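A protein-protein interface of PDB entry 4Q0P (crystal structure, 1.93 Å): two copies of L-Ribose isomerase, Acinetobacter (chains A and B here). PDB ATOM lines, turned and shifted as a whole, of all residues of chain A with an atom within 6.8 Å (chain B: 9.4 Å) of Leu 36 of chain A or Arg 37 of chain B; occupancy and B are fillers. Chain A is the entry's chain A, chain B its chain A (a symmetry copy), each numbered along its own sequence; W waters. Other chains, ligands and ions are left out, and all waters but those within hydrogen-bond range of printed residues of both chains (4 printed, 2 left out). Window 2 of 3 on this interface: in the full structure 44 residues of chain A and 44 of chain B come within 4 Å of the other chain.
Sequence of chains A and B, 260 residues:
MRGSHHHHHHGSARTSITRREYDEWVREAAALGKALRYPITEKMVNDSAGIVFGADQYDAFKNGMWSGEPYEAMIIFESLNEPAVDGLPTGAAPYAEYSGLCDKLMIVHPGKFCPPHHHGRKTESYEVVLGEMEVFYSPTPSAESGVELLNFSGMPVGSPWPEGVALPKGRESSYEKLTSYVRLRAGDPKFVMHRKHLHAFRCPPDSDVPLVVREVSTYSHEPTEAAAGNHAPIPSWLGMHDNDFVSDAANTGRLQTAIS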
ATOM      1  N   ALA A  30     -42.271  -4.929 -23.392  1.00  0.00           N
ATOM      2  CA  ALA A  30     -41.321  -5.338 -24.421  1.00  0.00           C
ATOM      3  C   ALA A  30     -41.043  -4.164 -25.365  1.00  0.00           C
ATOM      4  O   ALA A  30     -39.908  -3.955 -25.798  1.00  0.00           O
ATOM      5  CB  ALA A  30     -41.872  -6.533 -25.200  1.00  0.00           C
ATOM      6  N   ALA A  31     -42.086  -3.394 -25.673  1.00  0.00           N
ATOM      7  CA  ALA A  31     -41.948  -2.240 -26.556  1.00  0.00           C
ATOM      8  C   ALA A  31     -41.106  -1.180 -25.847  1.00  0.00           C
ATOM      9  O   ALA A  31     -40.259  -0.524 -26.461  1.00  0.00           O
ATOM     10  CB  ALA A  31     -43.337  -1.680 -26.922  1.00  0.00           C
ATOM     11  N   LEU A  32     -41.329  -1.021 -24.546  1.00  0.00           N
ATOM     12  CA  LEU A  32     -40.558  -0.045 -23.793  1.00  0.00           C
ATOM     13  C   LEU A  32     -39.086  -0.464 -23.826  1.00  0.00           C
ATOM     14  O   LEU A  32     -38.203   0.367 -24.015  1.00  0.00           O
ATOM     15  CB  LEU A  32     -41.062   0.040 -22.350  1.00  0.00           C
ATOM     16  CG  LEU A  32     -40.308   0.988 -21.408  1.00  0.00           C
ATOM     17  CD1 LEU A  32     -40.332   2.413 -21.949  1.00  0.00           C
ATOM     18  CD2 LEU A  32     -40.953   0.937 -20.031  1.00  0.00           C
ATOM     19  N   GLY A  33     -38.832  -1.759 -23.650  1.00  0.00           N
ATOM     20  CA  GLY A  33     -37.470  -2.260 -23.669  1.00  0.00           C
ATOM     21  C   GLY A  33     -36.800  -2.005 -25.004  1.00  0.00           C
ATOM     22  O   GLY A  33     -35.637  -1.598 -25.068  1.00  0.00           O
ATOM     23  N   LYS A  34     -37.537  -2.258 -26.078  1.00  0.00           N
ATOM     24  CA  LYS A  34     -37.027  -2.036 -27.419  1.00  0.00           C
ATOM     25  C   LYS A  34     -36.758  -0.558 -27.635  1.00  0.00           C
ATOM     26  O   LYS A  34     -35.758  -0.190 -28.250  1.00  0.00           O
ATOM     27  CB  LYS A  34     -38.020  -2.568 -28.448  1.00  0.00           C
ATOM     28  CG  LYS A  34     -38.056  -4.087 -28.452  1.00  0.00           C
ATOM     29  CD  LYS A  34     -38.904  -4.644 -29.565  1.00  0.00           C
ATOM     30  CE  LYS A  34     -38.718  -6.153 -29.642  1.00  0.00           C
ATOM     31  NZ  LYS A  34     -39.630  -6.773 -30.630  1.00  0.00           N
ATOM     32  N   ALA A  35     -37.637   0.295 -27.115  1.00  0.00           N
ATOM     33  CA  ALA A  35     -37.437   1.731 -27.248  1.00  0.00           C
ATOM     34  C   ALA A  35     -36.101   2.096 -26.605  1.00  0.00           C
ATOM     35  O   ALA A  35     -35.401   2.995 -27.067  1.00  0.00           O
ATOM     36  CB  ALA A  35     -38.570   2.491 -26.563  1.00  0.00           C
ATOM     37  N   LEU A  36     -35.753   1.390 -25.533  1.00  0.00           N
ATOM     38  CA  LEU A  36     -34.509   1.649 -24.817  1.00  0.00           C
ATOM     39  C   LEU A  36     -33.329   0.876 -25.404  1.00  0.00           C
ATOM     40  O   LEU A  36     -32.275   0.775 -24.784  1.00  0.00           O
ATOM     41  CB  LEU A  36     -34.685   1.313 -23.333  1.00  0.00           C
ATOM     42  CG  LEU A  36     -35.754   2.159 -22.622  1.00  0.00           C
ATOM     43  CD1 LEU A  36     -36.178   1.520 -21.306  1.00  0.00           C
ATOM     44  CD2 LEU A  36     -35.210   3.560 -22.398  1.00  0.00           C
ATOM     45  N   ARG A  37     -33.519   0.324 -26.595  1.00  0.00           N
ATOM     46  CA  ARG A  37     -32.466  -0.414 -27.290  1.00  0.00           C
ATOM     47  C   ARG A  37     -32.047  -1.747 -26.665  1.00  0.00           C
ATOM     48  O   ARG A  37     -30.973  -2.256 -26.984  1.00  0.00           O
ATOM     49  CB  ARG A  37     -31.208   0.455 -27.437  1.00  0.00           C
ATOM     50  CG  ARG A  37     -31.372   1.754 -28.215  1.00  0.00           C
ATOM     51  CD  ARG A  37     -30.048   2.534 -28.184  1.00  0.00           C
ATOM     52  NE  ARG A  37     -30.053   3.751 -28.997  1.00  0.00           N
ATOM     53  CZ  ARG A  37     -30.142   3.773 -30.325  1.00  0.00           C
ATOM     54  NH1 ARG A  37     -30.244   2.639 -31.010  1.00  0.00           N
ATOM     55  NH2 ARG A  37     -30.106   4.930 -30.974  1.00  0.00           N
ATOM     56  N   TYR A  38     -32.848  -2.314 -25.768  1.00  0.00           N
ATOM     57  CA  TYR A  38     -32.449  -3.605 -25.211  1.00  0.00           C
ATOM     58  C   TYR A  38     -32.799  -4.623 -26.297  1.00  0.00           C
ATOM     59  O   TYR A  38     -33.874  -4.560 -26.880  1.00  0.00           O
ATOM     60  CB  TYR A  38     -33.201  -3.933 -23.911  1.00  0.00           C
ATOM     61  CG  TYR A  38     -32.563  -5.087 -23.155  1.00  0.00           C
ATOM     62  CD1 TYR A  38     -31.399  -4.897 -22.401  1.00  0.00           C
ATOM     63  CD2 TYR A  38     -33.090  -6.375 -23.233  1.00  0.00           C
ATOM     64  CE1 TYR A  38     -30.778  -5.963 -21.740  1.00  0.00           C
ATOM     65  CE2 TYR A  38     -32.470  -7.456 -22.577  1.00  0.00           C
ATOM     66  CZ  TYR A  38     -31.318  -7.238 -21.835  1.00  0.00           C
ATOM     67  OH  TYR A  38     -30.704  -8.293 -21.190  1.00  0.00           O
ATOM     68  N   PRO A  39     -31.886  -5.561 -26.591  1.00  0.00           N
ATOM     69  CA  PRO A  39     -32.104  -6.585 -27.621  1.00  0.00           C
ATOM     70  C   PRO A  39     -33.117  -7.665 -27.257  1.00  0.00           C
ATOM     71  O   PRO A  39     -32.738  -8.774 -26.881  1.00  0.00           O
ATOM     72  CB  PRO A  39     -30.712  -7.163 -27.827  1.00  0.00           C
ATOM     73  CG  PRO A  39     -30.127  -7.092 -26.436  1.00  0.00           C
ATOM     74  CD  PRO A  39     -30.545  -5.697 -25.991  1.00  0.00           C
ATOM     75  N   LEU A 105     -33.330  -7.630 -18.745  1.00  0.00           N
ATOM     76  CA  LEU A 105     -33.918  -6.323 -18.550  1.00  0.00           C
ATOM     77  C   LEU A 105     -35.090  -6.591 -17.614  1.00  0.00           C
ATOM     78  O   LEU A 105     -35.860  -7.515 -17.852  1.00  0.00           O
ATOM     79  CB  LEU A 105     -34.442  -5.765 -19.878  1.00  0.00           C
ATOM     80  CG  LEU A 105     -34.757  -4.271 -19.800  1.00  0.00           C
ATOM     81  CD1 LEU A 105     -33.421  -3.520 -19.635  1.00  0.00           C
ATOM     82  CD2 LEU A 105     -35.494  -3.795 -21.058  1.00  0.00           C
ATOM     83  N   ILE A 107     -38.484  -4.932 -15.563  1.00  0.00           N
ATOM     84  CA  ILE A 107     -39.385  -3.791 -15.526  1.00  0.00           C
ATOM     85  C   ILE A 107     -40.325  -3.887 -14.332  1.00  0.00           C
ATOM     86  O   ILE A 107     -41.064  -4.862 -14.183  1.00  0.00           O
ATOM     87  CB  ILE A 107     -40.182  -3.681 -16.854  1.00  0.00           C
ATOM     88  CG1 ILE A 107     -39.196  -3.639 -18.029  1.00  0.00           C
ATOM     89  CG2 ILE A 107     -41.045  -2.428 -16.850  1.00  0.00           C
ATOM     90  CD1 ILE A 107     -39.836  -3.455 -19.390  1.00  0.00           C
ATOM     91  N   GLU A 127     -27.859  -1.668 -13.440  1.00  0.00           N
ATOM     92  CA  GLU A 127     -27.652  -0.488 -14.269  1.00  0.00           C
ATOM     93  C   GLU A 127     -29.054   0.036 -14.559  1.00  0.00           C
ATOM     94  O   GLU A 127     -29.811  -0.594 -15.299  1.00  0.00           O
ATOM     95  CB  GLU A 127     -26.966  -0.855 -15.584  1.00  0.00           C
ATOM     96  CG  GLU A 127     -26.744   0.332 -16.515  1.00  0.00           C
ATOM     97  CD  GLU A 127     -26.333  -0.092 -17.913  1.00  0.00           C
ATOM     98  OE1 GLU A 127     -25.485  -0.994 -18.026  1.00  0.00           O
ATOM     99  OE2 GLU A 127     -26.850   0.481 -18.894  1.00  0.00           O
ATOM    100  N   VAL A 128     -29.424   1.167 -13.968  1.00  0.00           N
ATOM    101  CA  VAL A 128     -30.757   1.700 -14.217  1.00  0.00           C
ATOM    102  C   VAL A 128     -30.783   2.332 -15.600  1.00  0.00           C
ATOM    103  O   VAL A 128     -29.881   3.094 -15.964  1.00  0.00           O
ATOM    104  CB  VAL A 128     -31.169   2.746 -13.147  1.00  0.00           C
ATOM    105  CG1 VAL A 128     -32.506   3.403 -13.527  1.00  0.00           C
ATOM    106  CG2 VAL A 128     -31.300   2.062 -11.789  1.00  0.00           C
ATOM    107  N   VAL A 129     -31.808   2.005 -16.378  1.00  0.00           N
ATOM    108  CA  VAL A 129     -31.927   2.555 -17.727  1.00  0.00           C
ATOM    109  C   VAL A 129     -32.976   3.654 -17.760  1.00  0.00           C
ATOM    110  O   VAL A 129     -32.794   4.682 -18.416  1.00  0.00           O
ATOM    111  CB  VAL A 129     -32.323   1.466 -18.739  1.00  0.00           C
ATOM    112  CG1 VAL A 129     -32.314   2.039 -20.160  1.00  0.00           C
ATOM    113  CG2 VAL A 129     -31.379   0.296 -18.616  1.00  0.00           C
ATOM    114  N   LEU A 130     -34.073   3.428 -17.045  1.00  0.00           N
ATOM    115  CA  LEU A 130     -35.165   4.388 -16.978  1.00  0.00           C
ATOM    116  C   LEU A 130     -35.761   4.351 -15.578  1.00  0.00           C
ATOM    117  O   LEU A 130     -35.849   3.279 -14.963  1.00  0.00           O
ATOM    118  CB  LEU A 130     -36.254   4.035 -18.000  1.00  0.00           C
ATOM    119  CG  LEU A 130     -37.392   5.047 -18.138  1.00  0.00           C
ATOM    120  CD1 LEU A 130     -36.873   6.257 -18.896  1.00  0.00           C
ATOM    121  CD2 LEU A 130     -38.581   4.420 -18.866  1.00  0.00           C
ATOM    122  N   ALA A 186     -30.132   6.432 -13.487  1.00  0.00           N
ATOM    123  CA  ALA A 186     -29.459   6.218 -14.761  1.00  0.00           C
ATOM    124  C   ALA A 186     -28.148   6.986 -14.736  1.00  0.00           C
ATOM    125  O   ALA A 186     -28.107   8.129 -14.292  1.00  0.00           O
ATOM    126  CB  ALA A 186     -30.338   6.713 -15.914  1.00  0.00           C
ATOM    127  N   GLY A 187     -27.070   6.356 -15.194  1.00  0.00           N
ATOM    128  CA  GLY A 187     -25.790   7.035 -15.216  1.00  0.00           C
ATOM    129  C   GLY A 187     -24.909   6.805 -14.003  1.00  0.00           C
ATOM    130  O   GLY A 187     -23.743   7.209 -14.000  1.00  0.00           O
ATOM    131  N   VAL A 212     -36.860   0.637 -15.217  1.00  0.00           N
ATOM    132  CA  VAL A 212     -36.294  -0.308 -16.178  1.00  0.00           C
ATOM    133  C   VAL A 212     -34.821  -0.470 -15.819  1.00  0.00           C
ATOM    134  O   VAL A 212     -34.036   0.482 -15.888  1.00  0.00           O
ATOM    135  CB  VAL A 212     -36.429   0.177 -17.646  1.00  0.00           C
ATOM    136  CG1 VAL A 212     -35.879  -0.891 -18.596  1.00  0.00           C
ATOM    137  CG2 VAL A 212     -37.890   0.451 -17.981  1.00  0.00           C
ATOM    138  N   ARG A 214     -31.167  -2.928 -16.133  1.00  0.00           N
ATOM    139  CA  ARG A 214     -30.428  -3.980 -16.794  1.00  0.00           C
ATOM    140  C   ARG A 214     -29.617  -4.710 -15.728  1.00  0.00           C
ATOM    141  O   ARG A 214     -28.826  -4.102 -15.005  1.00  0.00           O
ATOM    142  CB  ARG A 214     -29.467  -3.417 -17.846  1.00  0.00           C
ATOM    143  CG  ARG A 214     -28.624  -4.520 -18.498  1.00  0.00           C
ATOM    144  CD  ARG A 214     -27.517  -3.979 -19.394  1.00  0.00           C
ATOM    145  NE  ARG A 214     -28.019  -3.276 -20.572  1.00  0.00           N
ATOM    146  CZ  ARG A 214     -27.986  -3.762 -21.812  1.00  0.00           C
ATOM    147  NH1 ARG A 214     -28.462  -3.043 -22.818  1.00  0.00           N
ATOM    148  NH2 ARG A 214     -27.480  -4.964 -22.045  1.00  0.00           N
ATOM    149  N   ALA B  29     -15.807   9.729 -28.279  1.00  0.00           N
ATOM    150  CA  ALA B  29     -16.305   8.371 -28.086  1.00  0.00           C
ATOM    151  C   ALA B  29     -17.101   8.287 -26.792  1.00  0.00           C
ATOM    152  O   ALA B  29     -18.132   7.624 -26.733  1.00  0.00           O
ATOM    153  CB  ALA B  29     -15.149   7.382 -28.055  1.00  0.00           C
ATOM    154  N   ALA B  30     -16.617   8.956 -25.750  1.00  0.00           N
ATOM    155  CA  ALA B  30     -17.322   8.955 -24.473  1.00  0.00           C
ATOM    156  C   ALA B  30     -18.694   9.615 -24.638  1.00  0.00           C
ATOM    157  O   ALA B  30     -19.685   9.165 -24.060  1.00  0.00           O
ATOM    158  CB  ALA B  30     -16.496   9.691 -23.417  1.00  0.00           C
ATOM    159  N   ALA B  31     -18.746  10.679 -25.438  1.00  0.00           N
ATOM    160  CA  ALA B  31     -19.997  11.390 -25.683  1.00  0.00           C
ATOM    161  C   ALA B  31     -20.928  10.480 -26.482  1.00  0.00           C
ATOM    162  O   ALA B  31     -22.137  10.429 -26.234  1.00  0.00           O
ATOM    163  CB  ALA B  31     -19.724  12.700 -26.448  1.00  0.00           C
ATOM    164  N   LEU B  32     -20.362   9.746 -27.436  1.00  0.00           N
ATOM    165  CA  LEU B  32     -21.175   8.840 -28.232  1.00  0.00           C
ATOM    166  C   LEU B  32     -21.762   7.775 -27.302  1.00  0.00           C
ATOM    167  O   LEU B  32     -22.934   7.430 -27.406  1.00  0.00           O
ATOM    168  CB  LEU B  32     -20.335   8.190 -29.333  1.00  0.00           C
ATOM    169  CG  LEU B  32     -21.038   7.159 -30.225  1.00  0.00           C
ATOM    170  CD1 LEU B  32     -22.239   7.786 -30.924  1.00  0.00           C
ATOM    171  CD2 LEU B  32     -20.048   6.631 -31.251  1.00  0.00           C
ATOM    172  N   GLY B  33     -20.939   7.266 -26.387  1.00  0.00           N
ATOM    173  CA  GLY B  33     -21.397   6.254 -25.453  1.00  0.00           C
ATOM    174  C   GLY B  33     -22.527   6.768 -24.584  1.00  0.00           C
ATOM    175  O   GLY B  33     -23.518   6.073 -24.345  1.00  0.00           O
ATOM    176  N   LYS B  34     -22.369   7.993 -24.097  1.00  0.00           N
ATOM    177  CA  LYS B  34     -23.384   8.617 -23.267  1.00  0.00           C
ATOM    178  C   LYS B  34     -24.658   8.821 -24.068  1.00  0.00           C
ATOM    179  O   LYS B  34     -25.757   8.619 -23.553  1.00  0.00           O
ATOM    180  CB  LYS B  34     -22.865   9.942 -22.717  1.00  0.00           C
ATOM    181  CG  LYS B  34     -21.792   9.724 -21.663  1.00  0.00           C
ATOM    182  CD  LYS B  34     -21.375  11.004 -20.987  1.00  0.00           C
ATOM    183  CE  LYS B  34     -20.470  10.685 -19.805  1.00  0.00           C
ATOM    184  NZ  LYS B  34     -19.920  11.911 -19.184  1.00  0.00           N
ATOM    185  N   ALA B  35     -24.516   9.203 -25.334  1.00  0.00           N
ATOM    186  CA  ALA B  35     -25.684   9.390 -26.183  1.00  0.00           C
ATOM    187  C   ALA B  35     -26.451   8.071 -26.249  1.00  0.00           C
ATOM    188  O   ALA B  35     -27.678   8.055 -26.321  1.00  0.00           O
ATOM    189  CB  ALA B  35     -25.260   9.817 -27.585  1.00  0.00           C
ATOM    190  N   LEU B  36     -25.716   6.963 -26.224  1.00  0.00           N
ATOM    191  CA  LEU B  36     -26.325   5.640 -26.297  1.00  0.00           C
ATOM    192  C   LEU B  36     -26.727   5.108 -24.922  1.00  0.00           C
ATOM    193  O   LEU B  36     -27.015   3.926 -24.765  1.00  0.00           O
ATOM    194  CB  LEU B  36     -25.366   4.665 -26.989  1.00  0.00           C
ATOM    195  CG  LEU B  36     -25.028   5.044 -28.440  1.00  0.00           C
ATOM    196  CD1 LEU B  36     -23.786   4.310 -28.926  1.00  0.00           C
ATOM    197  CD2 LEU B  36     -26.224   4.735 -29.325  1.00  0.00           C
ATOM    198  N   ARG B  37     -26.732   5.987 -23.928  1.00  0.00           N
ATOM    199  CA  ARG B  37     -27.128   5.626 -22.569  1.00  0.00           C
ATOM    200  C   ARG B  37     -26.188   4.681 -21.817  1.00  0.00           C
ATOM    201  O   ARG B  37     -26.599   4.079 -20.826  1.00  0.00           O
ATOM    202  CB  ARG B  37     -28.530   4.997 -22.567  1.00  0.00           C
ATOM    203  CG  ARG B  37     -29.661   5.867 -23.100  1.00  0.00           C
ATOM    204  CD  ARG B  37     -30.964   5.054 -23.111  1.00  0.00           C
ATOM    205  NE  ARG B  37     -32.146   5.825 -23.499  1.00  0.00           N
ATOM    206  CZ  ARG B  37     -32.666   6.823 -22.788  1.00  0.00           C
ATOM    207  NH1 ARG B  37     -32.106   7.191 -21.641  1.00  0.00           N
ATOM    208  NH2 ARG B  37     -33.761   7.441 -23.212  1.00  0.00           N
ATOM    209  N   TYR B  38     -24.950   4.515 -22.270  1.00  0.00           N
ATOM    210  CA  TYR B  38     -24.054   3.638 -21.517  1.00  0.00           C
ATOM    211  C   TYR B  38     -23.599   4.479 -20.324  1.00  0.00           C
ATOM    212  O   TYR B  38     -23.256   5.644 -20.483  1.00  0.00           O
ATOM    213  CB  TYR B  38     -22.842   3.193 -22.350  1.00  0.00           C
ATOM    214  CG  TYR B  38     -22.098   2.034 -21.707  1.00  0.00           C
ATOM    215  CD1 TYR B  38     -22.596   0.728 -21.787  1.00  0.00           C
ATOM    216  CD2 TYR B  38     -20.929   2.246 -20.979  1.00  0.00           C
ATOM    217  CE1 TYR B  38     -21.945  -0.339 -21.158  1.00  0.00           C
ATOM    218  CE2 TYR B  38     -20.268   1.181 -20.337  1.00  0.00           C
ATOM    219  CZ  TYR B  38     -20.784  -0.104 -20.434  1.00  0.00           C
ATOM    220  OH  TYR B  38     -20.142  -1.154 -19.807  1.00  0.00           O
ATOM    221  N   PRO B  39     -23.607   3.901 -19.113  1.00  0.00           N
ATOM    222  CA  PRO B  39     -23.200   4.610 -17.893  1.00  0.00           C
ATOM    223  C   PRO B  39     -21.706   4.882 -17.768  1.00  0.00           C
ATOM    224  O   PRO B  39     -21.001   4.176 -17.047  1.00  0.00           O
ATOM    225  CB  PRO B  39     -23.702   3.695 -16.785  1.00  0.00           C
ATOM    226  CG  PRO B  39     -23.511   2.325 -17.390  1.00  0.00           C
ATOM    227  CD  PRO B  39     -24.047   2.528 -18.801  1.00  0.00           C
ATOM    228  N   ILE B  40     -21.232   5.906 -18.465  1.00  0.00           N
ATOM    229  CA  ILE B  40     -19.823   6.273 -18.427  1.00  0.00           C
ATOM    230  C   ILE B  40     -19.583   7.322 -17.352  1.00  0.00           C
ATOM    231  O   ILE B  40     -20.176   8.401 -17.378  1.00  0.00           O
ATOM    232  CB  ILE B  40     -19.356   6.824 -19.798  1.00  0.00           C
ATOM    233  CG1 ILE B  40     -19.434   5.708 -20.848  1.00  0.00           C
ATOM    234  CG2 ILE B  40     -17.925   7.365 -19.697  1.00  0.00           C
ATOM    235  CD1 ILE B  40     -19.015   6.125 -22.232  1.00  0.00           C
ATOM    236  N   SER B  79     -17.269  -0.269 -17.321  1.00  0.00           N
ATOM    237  CA  SER B  79     -18.145   0.156 -16.233  1.00  0.00           C
ATOM    238  C   SER B  79     -18.111  -0.819 -15.070  1.00  0.00           C
ATOM    239  O   SER B  79     -18.452  -0.460 -13.942  1.00  0.00           O
ATOM    240  CB  SER B  79     -19.595   0.297 -16.724  1.00  0.00           C
ATOM    241  OG  SER B  79     -20.164  -0.964 -17.042  1.00  0.00           O
ATOM    242  N   ASP B 103     -18.279  -5.601 -17.566  1.00  0.00           N
ATOM    243  CA  ASP B 103     -19.181  -4.931 -18.502  1.00  0.00           C
ATOM    244  C   ASP B 103     -18.421  -3.749 -19.074  1.00  0.00           C
ATOM    245  O   ASP B 103     -17.872  -2.949 -18.326  1.00  0.00           O
ATOM    246  CB  ASP B 103     -20.428  -4.420 -17.760  1.00  0.00           C
ATOM    247  CG  ASP B 103     -21.580  -4.073 -18.698  1.00  0.00           C
ATOM    248  OD1 ASP B 103     -21.342  -3.461 -19.760  1.00  0.00           O
ATOM    249  OD2 ASP B 103     -22.740  -4.405 -18.358  1.00  0.00           O
ATOM    250  N   LEU B 105     -18.038  -0.942 -22.780  1.00  0.00           N
ATOM    251  CA  LEU B 105     -18.517  -0.460 -24.058  1.00  0.00           C
ATOM    252  C   LEU B 105     -17.252  -0.348 -24.899  1.00  0.00           C
ATOM    253  O   LEU B 105     -16.259   0.204 -24.436  1.00  0.00           O
ATOM    254  CB  LEU B 105     -19.153   0.926 -23.905  1.00  0.00           C
ATOM    255  CG  LEU B 105     -19.971   1.331 -25.131  1.00  0.00           C
ATOM    256  CD1 LEU B 105     -21.206   0.411 -25.193  1.00  0.00           C
ATOM    257  CD2 LEU B 105     -20.397   2.803 -25.050  1.00  0.00           C
ATOM    258  N   GLU B 127     -23.155  -7.497 -27.727  1.00  0.00           N
ATOM    259  CA  GLU B 127     -24.442  -6.868 -27.992  1.00  0.00           C
ATOM    260  C   GLU B 127     -24.104  -5.607 -28.781  1.00  0.00           C
ATOM    261  O   GLU B 127     -23.534  -4.665 -28.230  1.00  0.00           O
ATOM    262  CB  GLU B 127     -25.140  -6.479 -26.690  1.00  0.00           C
ATOM    263  CG  GLU B 127     -26.484  -5.787 -26.895  1.00  0.00           C
ATOM    264  CD  GLU B 127     -27.016  -5.159 -25.621  1.00  0.00           C
ATOM    265  OE1 GLU B 127     -26.936  -5.814 -24.567  1.00  0.00           O
ATOM    266  OE2 GLU B 127     -27.522  -4.019 -25.676  1.00  0.00           O
ATOM    267  N   VAL B 128     -24.424  -5.583 -30.071  1.00  0.00           N
ATOM    268  CA  VAL B 128     -24.117  -4.398 -30.860  1.00  0.00           C
ATOM    269  C   VAL B 128     -25.120  -3.306 -30.519  1.00  0.00           C
ATOM    270  O   VAL B 128     -26.329  -3.553 -30.466  1.00  0.00           O
ATOM    271  CB  VAL B 128     -24.152  -4.694 -32.383  1.00  0.00           C
ATOM    272  CG1 VAL B 128     -23.983  -3.394 -33.186  1.00  0.00           C
ATOM    273  CG2 VAL B 128     -23.032  -5.667 -32.740  1.00  0.00           C
ATOM    274  N   VAL B 129     -24.618  -2.102 -30.271  1.00  0.00           N
ATOM    275  CA  VAL B 129     -25.494  -0.983 -29.931  1.00  0.00           C
ATOM    276  C   VAL B 129     -25.656  -0.055 -31.123  1.00  0.00           C
ATOM    277  O   VAL B 129     -26.750   0.446 -31.391  1.00  0.00           O
ATOM    278  CB  VAL B 129     -24.932  -0.175 -28.750  1.00  0.00           C
ATOM    279  CG1 VAL B 129     -25.930   0.910 -28.330  1.00  0.00           C
ATOM    280  CG2 VAL B 129     -24.623  -1.104 -27.603  1.00  0.00           C
ATOM    281  N   VAL B 212     -20.222   0.364 -32.096  1.00  0.00           N
ATOM    282  CA  VAL B 212     -20.301   0.494 -30.642  1.00  0.00           C
ATOM    283  C   VAL B 212     -20.901  -0.806 -30.118  1.00  0.00           C
ATOM    284  O   VAL B 212     -22.051  -1.148 -30.417  1.00  0.00           O
ATOM    285  CB  VAL B 212     -21.173   1.697 -30.194  1.00  0.00           C
ATOM    286  CG1 VAL B 212     -21.154   1.810 -28.667  1.00  0.00           C
ATOM    287  CG2 VAL B 212     -20.647   2.989 -30.807  1.00  0.00           C
ATOM    288  N   ARG B 214     -21.471  -3.517 -26.679  1.00  0.00           N
ATOM    289  CA  ARG B 214     -21.452  -3.734 -25.250  1.00  0.00           C
ATOM    290  C   ARG B 214     -20.974  -5.163 -25.012  1.00  0.00           C
ATOM    291  O   ARG B 214     -21.556  -6.121 -25.523  1.00  0.00           O
ATOM    292  CB  ARG B 214     -22.846  -3.571 -24.637  1.00  0.00           C
ATOM    293  CG  ARG B 214     -22.848  -3.875 -23.134  1.00  0.00           C
ATOM    294  CD  ARG B 214     -24.248  -3.927 -22.535  1.00  0.00           C
ATOM    295  NE  ARG B 214     -24.935  -2.638 -22.561  1.00  0.00           N
ATOM    296  CZ  ARG B 214     -25.137  -1.868 -21.492  1.00  0.00           C
ATOM    297  NH1 ARG B 214     -25.778  -0.716 -21.618  1.00  0.00           N
ATOM    298  NH2 ARG B 214     -24.698  -2.250 -20.302  1.00  0.00           N
HETATM  299  O   HOH W   1     -30.632   5.578 -19.597  1.00  0.00           O
HETATM  300  O   HOH W   2     -28.499   2.402 -19.721  1.00  0.00           O
HETATM  301  O   HOH W   3     -29.133  -0.080 -30.435  1.00  0.00           O
HETATM  302  O   HOH W   4     -28.234  -1.984 -27.239  1.00  0.00           O
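Water W1 bridges O of Val 129 of chain A (2.6 Å) and NH1 of Arg 37 of chain B (3.0 Å).
Water W3 lies within hydrogen-bond range of the backbone carbonyl oxygen (O) of Val 129 of chain B (2.6 Å) and the guanidinium group (NH1) of Arg 37 of chain A (3.0 Å).
Water W4 lies within hydrogen-bond range of OE2 of Glu 127 of chain B (2.7 Å) and O of Arg 37 of chain A (2.8 Å).
Water W2 lies within hydrogen-bond range of OE2 of Glu 127 of chain A and O of Arg 37 of chain B.
NE of Arg 37 of chain B touches CD2 of Leu 36 of chain A, at 3.97 Å.
Arg 37 of chain A touches Leu 36 of chain B.
CD of Pro 39 of chain A touches OE2 of Glu 127 of chain B, at 3.5 Å.
OE2 of Glu 127 of chain A touches CD of Pro 39 of chain B (3.5 Å).
Leu 36 of chain A touches Arg 37 of chain B, and with the chains exchanged Arg 37 of chain A touches Leu 36 of chain B.
Pro 39 of chain A touches Glu 127 of chain B, and with the chains exchanged Glu 127 of chain A touches Pro 39 of chain B.
Glu 127 of chain A touches Arg 214 of chain B, and with the chains exchanged Arg 214 of chain A touches Glu 127 of chain B.
Arg 214 of chain A touches its own counterpart, Arg 214 of chain B.
16 positions are printed for both chains.
Of the 7 pairs that touch across the chains among the printed residues, 7 have their exchanged pair printed and touching as well.
Ala 31 of chain A touches none of the printed residues of chain B.
No residue of chain B comes within 4 Å of Ala 35 of chain A.
Of chain B, only Arg 37 comes within 4 Å of Leu 36 of chain A.
Printed residues of chain B within 4 Å of Arg 37 of chain A: Leu 36.
Printed residues of chain B within 4 Å of Arg 214 of chain A: Glu 127 (2.7 Å) and Arg 214 (3.3 Å).
Ala 30 of chain B touches none of the printed residues of chain A.
The nearest residue of chain A that does not touch Arg 37 of chain B is Glu 127 of chain A (4.1 Å).
The guanidinium group of Arg 214 of chain A is in salt-bridge range of the side-chain carboxylate of Glu 127 of chain B.
NH2 of Arg 214 of chain A lies close to NE of Arg 214 of chain B, at 3.5 Å.
The guanidinium group (NH2) of Arg 214 of chain B lies within salt-bridge range of the side-chain carboxylate (OE1) of Glu 127 of chain A, at 2.7 Å.
Printed residues of chain A that touch a printed residue of chain B: Leu 36, Arg 37, Pro 39, Glu 127 and Arg 214.
The backbone carbonyl oxygen of Glu 127 of chain A sits at hydrogen-bond distance from the backbone NH of Arg 214 of chain A, at 2.8 Å.
The backbone carbonyl oxygen (O) of Glu 127 of chain B sits at hydrogen-bond distance from the backbone NH (N) of Arg 214 of chain B (2.8 Å).
The side-chain carboxylate (OD2) of Asp 103 of chain B is in salt-bridge range of the guanidinium group (NH2) of Arg 214 of chain B, at 3.5 Å.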
